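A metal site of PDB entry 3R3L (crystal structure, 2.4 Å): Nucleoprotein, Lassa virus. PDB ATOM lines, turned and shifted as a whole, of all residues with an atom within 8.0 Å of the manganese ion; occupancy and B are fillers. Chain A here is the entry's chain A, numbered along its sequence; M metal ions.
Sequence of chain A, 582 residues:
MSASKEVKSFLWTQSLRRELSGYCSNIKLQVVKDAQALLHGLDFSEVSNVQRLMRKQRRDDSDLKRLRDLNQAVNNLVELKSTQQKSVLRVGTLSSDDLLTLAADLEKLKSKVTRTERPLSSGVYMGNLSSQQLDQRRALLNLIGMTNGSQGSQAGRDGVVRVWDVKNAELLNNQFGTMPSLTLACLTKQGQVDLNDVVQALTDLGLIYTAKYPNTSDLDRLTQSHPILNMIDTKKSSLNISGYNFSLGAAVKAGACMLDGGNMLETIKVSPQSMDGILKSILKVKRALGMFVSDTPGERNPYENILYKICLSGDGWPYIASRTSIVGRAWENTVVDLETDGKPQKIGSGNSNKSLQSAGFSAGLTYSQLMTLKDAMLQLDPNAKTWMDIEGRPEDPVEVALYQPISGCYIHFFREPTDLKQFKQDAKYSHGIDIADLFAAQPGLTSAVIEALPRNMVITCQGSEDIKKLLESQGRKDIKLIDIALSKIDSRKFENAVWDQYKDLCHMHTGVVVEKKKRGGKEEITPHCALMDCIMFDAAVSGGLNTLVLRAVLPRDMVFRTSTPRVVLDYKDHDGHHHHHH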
ATOM      1  N   MET A 388      19.085 -26.090  -9.440  1.00  0.00           N
ATOM      2  CA  MET A 388      19.628 -27.401  -9.786  1.00  0.00           C
ATOM      3  C   MET A 388      19.554 -27.638 -11.297  1.00  0.00           C
ATOM      4  O   MET A 388      18.673 -27.109 -11.985  1.00  0.00           O
ATOM      5  CB  MET A 388      18.912 -28.531  -9.033  1.00  0.00           C
ATOM      6  CG  MET A 388      19.620 -29.882  -9.100  1.00  0.00           C
ATOM      7  SD  MET A 388      18.816 -31.173  -8.135  1.00  0.00           S
ATOM      8  CE  MET A 388      19.756 -32.609  -8.630  1.00  0.00           C
ATOM      9  N   ASP A 389      20.507 -28.426 -11.796  1.00  0.00           N
ATOM     10  CA  ASP A 389      20.646 -28.718 -13.224  1.00  0.00           C
ATOM     11  C   ASP A 389      21.503 -29.968 -13.404  1.00  0.00           C
ATOM     12  O   ASP A 389      22.514 -30.129 -12.717  1.00  0.00           O
ATOM     13  CB  ASP A 389      21.313 -27.540 -13.937  1.00  0.00           C
ATOM     14  CG  ASP A 389      21.042 -27.522 -15.420  1.00  0.00           C
ATOM     15  OD1 ASP A 389      21.901 -27.985 -16.199  1.00  0.00           O
ATOM     16  OD2 ASP A 389      19.955 -27.035 -15.821  1.00  0.00           O
ATOM     17  N   ILE A 390      21.098 -30.854 -14.320  1.00  0.00           N
ATOM     18  CA  ILE A 390      21.843 -32.070 -14.610  1.00  0.00           C
ATOM     19  C   ILE A 390      22.175 -32.237 -16.089  1.00  0.00           C
ATOM     20  O   ILE A 390      21.397 -31.830 -16.953  1.00  0.00           O
ATOM     21  CB  ILE A 390      21.101 -33.361 -14.134  1.00  0.00           C
ATOM     22  CG1 ILE A 390      19.636 -33.364 -14.622  1.00  0.00           C
ATOM     23  CG2 ILE A 390      21.191 -33.496 -12.630  1.00  0.00           C
ATOM     24  CD1 ILE A 390      18.998 -34.731 -14.689  1.00  0.00           C
ATOM     25  N   GLU A 391      23.329 -32.834 -16.356  1.00  0.00           N
ATOM     26  CA  GLU A 391      23.668 -33.279 -17.705  1.00  0.00           C
ATOM     27  C   GLU A 391      23.623 -34.793 -17.741  1.00  0.00           C
ATOM     28  O   GLU A 391      23.920 -35.456 -16.752  1.00  0.00           O
ATOM     29  CB  GLU A 391      25.046 -32.746 -18.145  1.00  0.00           C
ATOM     30  CG  GLU A 391      25.085 -31.248 -18.425  1.00  0.00           C
ATOM     31  CD  GLU A 391      24.081 -30.788 -19.472  1.00  0.00           C
ATOM     32  OE1 GLU A 391      23.885 -31.494 -20.482  1.00  0.00           O
ATOM     33  OE2 GLU A 391      23.492 -29.697 -19.299  1.00  0.00           O
ATOM     34  N   GLY A 392      23.245 -35.338 -18.890  1.00  0.00           N
ATOM     35  CA  GLY A 392      22.963 -36.759 -19.012  1.00  0.00           C
ATOM     36  C   GLY A 392      21.527 -37.043 -18.602  1.00  0.00           C
ATOM     37  O   GLY A 392      20.877 -36.209 -17.949  1.00  0.00           O
ATOM     38  N   GLU A 399      26.665 -35.225 -14.821  1.00  0.00           N
ATOM     39  CA  GLU A 399      27.042 -33.986 -14.164  1.00  0.00           C
ATOM     40  C   GLU A 399      25.861 -33.411 -13.404  1.00  0.00           C
ATOM     41  O   GLU A 399      24.760 -33.295 -13.952  1.00  0.00           O
ATOM     42  CB  GLU A 399      27.574 -32.970 -15.189  1.00  0.00           C
ATOM     43  CG  GLU A 399      28.174 -31.720 -14.562  1.00  0.00           C
ATOM     44  CD  GLU A 399      28.728 -30.761 -15.606  1.00  0.00           C
ATOM     45  OE1 GLU A 399      27.961 -30.367 -16.513  1.00  0.00           O
ATOM     46  OE2 GLU A 399      29.906 -30.399 -15.505  1.00  0.00           O
ATOM     47  N   SER A 430      25.139 -32.131 -26.288  1.00  0.00           N
ATOM     48  CA  SER A 430      24.892 -31.452 -25.009  1.00  0.00           C
ATOM     49  C   SER A 430      26.143 -31.042 -24.226  1.00  0.00           C
ATOM     50  O   SER A 430      26.464 -29.860 -24.162  1.00  0.00           O
ATOM     51  CB  SER A 430      23.946 -32.285 -24.129  1.00  0.00           C
ATOM     52  OG  SER A 430      23.702 -31.648 -22.897  1.00  0.00           O
ATOM     53  N   HIS A 431      26.829 -32.006 -23.625  1.00  0.00           N
ATOM     54  CA  HIS A 431      27.920 -31.709 -22.679  1.00  0.00           C
ATOM     55  C   HIS A 431      29.350 -31.829 -23.210  1.00  0.00           C
ATOM     56  O   HIS A 431      30.265 -31.226 -22.645  1.00  0.00           O
ATOM     57  CB  HIS A 431      27.761 -32.490 -21.373  1.00  0.00           C
ATOM     58  CG  HIS A 431      27.420 -33.940 -21.547  1.00  0.00           C
ATOM     59  ND1 HIS A 431      28.270 -34.838 -22.169  1.00  0.00           N
ATOM     60  CD2 HIS A 431      26.337 -34.652 -21.169  1.00  0.00           C
ATOM     61  CE1 HIS A 431      27.718 -36.032 -22.163  1.00  0.00           C
ATOM     62  NE2 HIS A 431      26.541 -35.954 -21.569  1.00  0.00           N
ATOM     63  N   GLN A 462      15.301 -24.980 -14.723  1.00  0.00           N
ATOM     64  CA  GLN A 462      14.811 -24.963 -16.094  1.00  0.00           C
ATOM     65  C   GLN A 462      14.419 -26.387 -16.505  1.00  0.00           C
ATOM     66  O   GLN A 462      15.277 -27.249 -16.707  1.00  0.00           O
ATOM     67  CB  GLN A 462      15.867 -24.387 -17.039  1.00  0.00           C
ATOM     68  CG  GLN A 462      15.564 -24.500 -18.540  1.00  0.00           C
ATOM     69  CD  GLN A 462      14.441 -23.596 -19.008  1.00  0.00           C
ATOM     70  OE1 GLN A 462      14.161 -22.556 -18.401  1.00  0.00           O
ATOM     71  NE2 GLN A 462      13.789 -23.985 -20.100  1.00  0.00           N
ATOM     72  N   ASP A 466      12.648 -33.521 -15.715  1.00  0.00           N
ATOM     73  CA  ASP A 466      13.948 -34.159 -15.498  1.00  0.00           C
ATOM     74  C   ASP A 466      14.399 -34.224 -14.031  1.00  0.00           C
ATOM     75  O   ASP A 466      14.722 -35.310 -13.533  1.00  0.00           O
ATOM     76  CB  ASP A 466      15.017 -33.463 -16.344  1.00  0.00           C
ATOM     77  CG  ASP A 466      14.851 -31.955 -16.370  1.00  0.00           C
ATOM     78  OD1 ASP A 466      13.915 -31.464 -17.051  1.00  0.00           O
ATOM     79  OD2 ASP A 466      15.652 -31.251 -15.703  1.00  0.00           O
ATOM     80  N   ILE A 467      14.421 -33.080 -13.352  1.00  0.00           N
ATOM     81  CA  ILE A 467      14.853 -32.984 -11.950  1.00  0.00           C
ATOM     82  C   ILE A 467      13.936 -33.815 -11.041  1.00  0.00           C
ATOM     83  O   ILE A 467      14.395 -34.432 -10.073  1.00  0.00           O
ATOM     84  CB  ILE A 467      14.895 -31.502 -11.453  1.00  0.00           C
ATOM     85  CG1 ILE A 467      15.683 -30.600 -12.416  1.00  0.00           C
ATOM     86  CG2 ILE A 467      15.435 -31.404 -10.026  1.00  0.00           C
ATOM     87  CD1 ILE A 467      17.184 -30.866 -12.487  1.00  0.00           C
ATOM     88  N   ARG A 492      19.718 -18.386 -22.383  1.00  0.00           N
ATOM     89  CA  ARG A 492      21.130 -18.320 -22.723  1.00  0.00           C
ATOM     90  C   ARG A 492      21.555 -16.933 -23.200  1.00  0.00           C
ATOM     91  O   ARG A 492      22.345 -16.795 -24.148  1.00  0.00           O
ATOM     92  CB  ARG A 492      21.501 -19.411 -23.736  1.00  0.00           C
ATOM     93  CG  ARG A 492      21.170 -20.821 -23.237  1.00  0.00           C
ATOM     94  CD  ARG A 492      21.958 -21.907 -23.935  1.00  0.00           C
ATOM     95  NE  ARG A 492      21.782 -23.178 -23.229  1.00  0.00           N
ATOM     96  CZ  ARG A 492      22.588 -23.637 -22.274  1.00  0.00           C
ATOM     97  NH1 ARG A 492      23.654 -22.948 -21.905  1.00  0.00           N
ATOM     98  NH2 ARG A 492      22.323 -24.791 -21.698  1.00  0.00           N
ATOM     99  N   PRO A 527      29.176 -26.104 -25.379  1.00  0.00           N
ATOM    100  CA  PRO A 527      28.760 -27.266 -24.585  1.00  0.00           C
ATOM    101  C   PRO A 527      28.004 -26.879 -23.315  1.00  0.00           C
ATOM    102  O   PRO A 527      28.320 -25.856 -22.699  1.00  0.00           O
ATOM    103  CB  PRO A 527      30.085 -27.937 -24.222  1.00  0.00           C
ATOM    104  CG  PRO A 527      31.029 -27.527 -25.278  1.00  0.00           C
ATOM    105  CD  PRO A 527      30.629 -26.138 -25.675  1.00  0.00           C
ATOM    106  N   HIS A 528      27.018 -27.685 -22.936  1.00  0.00           N
ATOM    107  CA  HIS A 528      26.200 -27.425 -21.754  1.00  0.00           C
ATOM    108  C   HIS A 528      26.834 -27.973 -20.480  1.00  0.00           C
ATOM    109  O   HIS A 528      27.145 -29.166 -20.383  1.00  0.00           O
ATOM    110  CB  HIS A 528      24.776 -27.996 -21.916  1.00  0.00           C
ATOM    111  CG  HIS A 528      24.030 -27.463 -23.096  1.00  0.00           C
ATOM    112  ND1 HIS A 528      23.053 -28.194 -23.738  1.00  0.00           N
ATOM    113  CD2 HIS A 528      24.121 -26.287 -23.762  1.00  0.00           C
ATOM    114  CE1 HIS A 528      22.570 -27.488 -24.742  1.00  0.00           C
ATOM    115  NE2 HIS A 528      23.195 -26.323 -24.776  1.00  0.00           N
ATOM    116  N   CYS A 529      27.009 -27.072 -19.521  1.00  0.00           N
ATOM    117  CA  CYS A 529      27.561 -27.387 -18.218  1.00  0.00           C
ATOM    118  C   CYS A 529      26.462 -27.176 -17.182  1.00  0.00           C
ATOM    119  O   CYS A 529      25.742 -26.179 -17.229  1.00  0.00           O
ATOM    120  CB  CYS A 529      28.750 -26.470 -17.922  1.00  0.00           C
ATOM    121  SG  CYS A 529      29.514 -26.637 -16.292  1.00  0.00           S
ATOM    122  N   ALA A 530      26.342 -28.121 -16.257  1.00  0.00           N
ATOM    123  CA  ALA A 530      25.294 -28.080 -15.229  1.00  0.00           C
ATOM    124  C   ALA A 530      25.414 -26.857 -14.340  1.00  0.00           C
ATOM    125  O   ALA A 530      24.423 -26.185 -14.049  1.00  0.00           O
ATOM    126  CB  ALA A 530      25.309 -29.351 -14.401  1.00  0.00           C
ATOM    127  N   LEU A 531      26.637 -26.576 -13.899  1.00  0.00           N
ATOM    128  CA  LEU A 531      26.943 -25.450 -13.023  1.00  0.00           C
ATOM    129  C   LEU A 531      26.795 -24.112 -13.745  1.00  0.00           C
ATOM    130  O   LEU A 531      26.212 -23.177 -13.200  1.00  0.00           O
ATOM    131  CB  LEU A 531      28.350 -25.588 -12.442  1.00  0.00           C
ATOM    132  CG  LEU A 531      28.945 -24.426 -11.645  1.00  0.00           C
ATOM    133  CD1 LEU A 531      28.177 -24.187 -10.348  1.00  0.00           C
ATOM    134  CD2 LEU A 531      30.430 -24.679 -11.369  1.00  0.00           C
ATOM    135  N   MET A 532      27.313 -24.035 -14.972  1.00  0.00           N
ATOM    136  CA  MET A 532      27.218 -22.793 -15.751  1.00  0.00           C
ATOM    137  C   MET A 532      25.781 -22.504 -16.176  1.00  0.00           C
ATOM    138  O   MET A 532      25.398 -21.343 -16.326  1.00  0.00           O
ATOM    139  CB  MET A 532      28.164 -22.810 -16.952  1.00  0.00           C
ATOM    140  CG  MET A 532      29.628 -23.092 -16.619  1.00  0.00           C
ATOM    141  SD  MET A 532      30.391 -21.947 -15.458  1.00  0.00           S
ATOM    142  CE  MET A 532      31.643 -23.006 -14.736  1.00  0.00           C
ATOM    143  N   ASP A 533      24.989 -23.567 -16.351  1.00  0.00           N
ATOM    144  CA  ASP A 533      23.549 -23.428 -16.586  1.00  0.00           C
ATOM    145  C   ASP A 533      22.853 -22.823 -15.378  1.00  0.00           C
ATOM    146  O   ASP A 533      22.074 -21.885 -15.513  1.00  0.00           O
ATOM    147  CB  ASP A 533      22.917 -24.775 -16.944  1.00  0.00           C
ATOM    148  CG  ASP A 533      23.010 -25.092 -18.424  1.00  0.00           C
ATOM    149  OD1 ASP A 533      23.310 -24.187 -19.232  1.00  0.00           O
ATOM    150  OD2 ASP A 533      22.766 -26.270 -18.794  1.00  0.00           O
ATOM    151  N   CYS A 534      23.146 -23.357 -14.187  1.00  0.00           N
ATOM    152  CA  CYS A 534      22.604 -22.837 -12.938  1.00  0.00           C
ATOM    153  C   CYS A 534      22.849 -21.328 -12.781  1.00  0.00           C
ATOM    154  O   CYS A 534      21.937 -20.566 -12.460  1.00  0.00           O
ATOM    155  CB  CYS A 534      23.189 -23.592 -11.744  1.00  0.00           C
ATOM    156  SG  CYS A 534      22.428 -25.205 -11.407  1.00  0.00           S
ATOM    157  N   PHE A 537      21.020 -19.326 -15.782  1.00  0.00           N
ATOM    158  CA  PHE A 537      19.562 -19.334 -15.594  1.00  0.00           C
ATOM    159  C   PHE A 537      19.148 -18.382 -14.477  1.00  0.00           C
ATOM    160  O   PHE A 537      18.041 -17.861 -14.488  1.00  0.00           O
ATOM    161  CB  PHE A 537      19.026 -20.749 -15.298  1.00  0.00           C
ATOM    162  CG  PHE A 537      19.186 -21.735 -16.427  1.00  0.00           C
ATOM    163  CD1 PHE A 537      19.219 -21.308 -17.761  1.00  0.00           C
ATOM    164  CD2 PHE A 537      19.271 -23.094 -16.172  1.00  0.00           C
ATOM    165  CE1 PHE A 537      19.362 -22.225 -18.798  1.00  0.00           C
ATOM    166  CE2 PHE A 537      19.396 -24.024 -17.200  1.00  0.00           C
ATOM    167  CZ  PHE A 537      19.447 -23.586 -18.523  1.00  0.00           C
HETATM  168 MN    MN M   1      22.146 -28.167 -18.082  1.00  0.00          MN
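The backbone NH (N) of Asp 389 lies close to the side-chain sulfur (SG) of Cys 534 (3.8 Å).
NH2 of Arg 492 is in salt-bridge range of OD1 of Asp 533 (2.7 Å).
The side-chain hydroxyl (OG) of Ser 430 is in hydrogen-bond range of the side-chain carboxylate (OE1) of Glu 391, at 2.4 Å.
The backbone NH (N) of Glu 391 is in hydrogen-bond range of the backbone carbonyl oxygen (O) of Glu 399.
Merely in contact with the manganese ion: Ile 390.
Four residues have an atom within 4 Å of the manganese ion: Asp 389, Ile 390, Glu 391 and Asp 533.
The manganese ion is bound by the side-chain carboxylate of Asp 389 (1.9 Å), the side-chain carboxylate of Asp 533 (2.1 Å) and the side-chain carboxylate of Glu 391 (2.4 Å).
The manganese ion has three donor atoms within binding distance.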
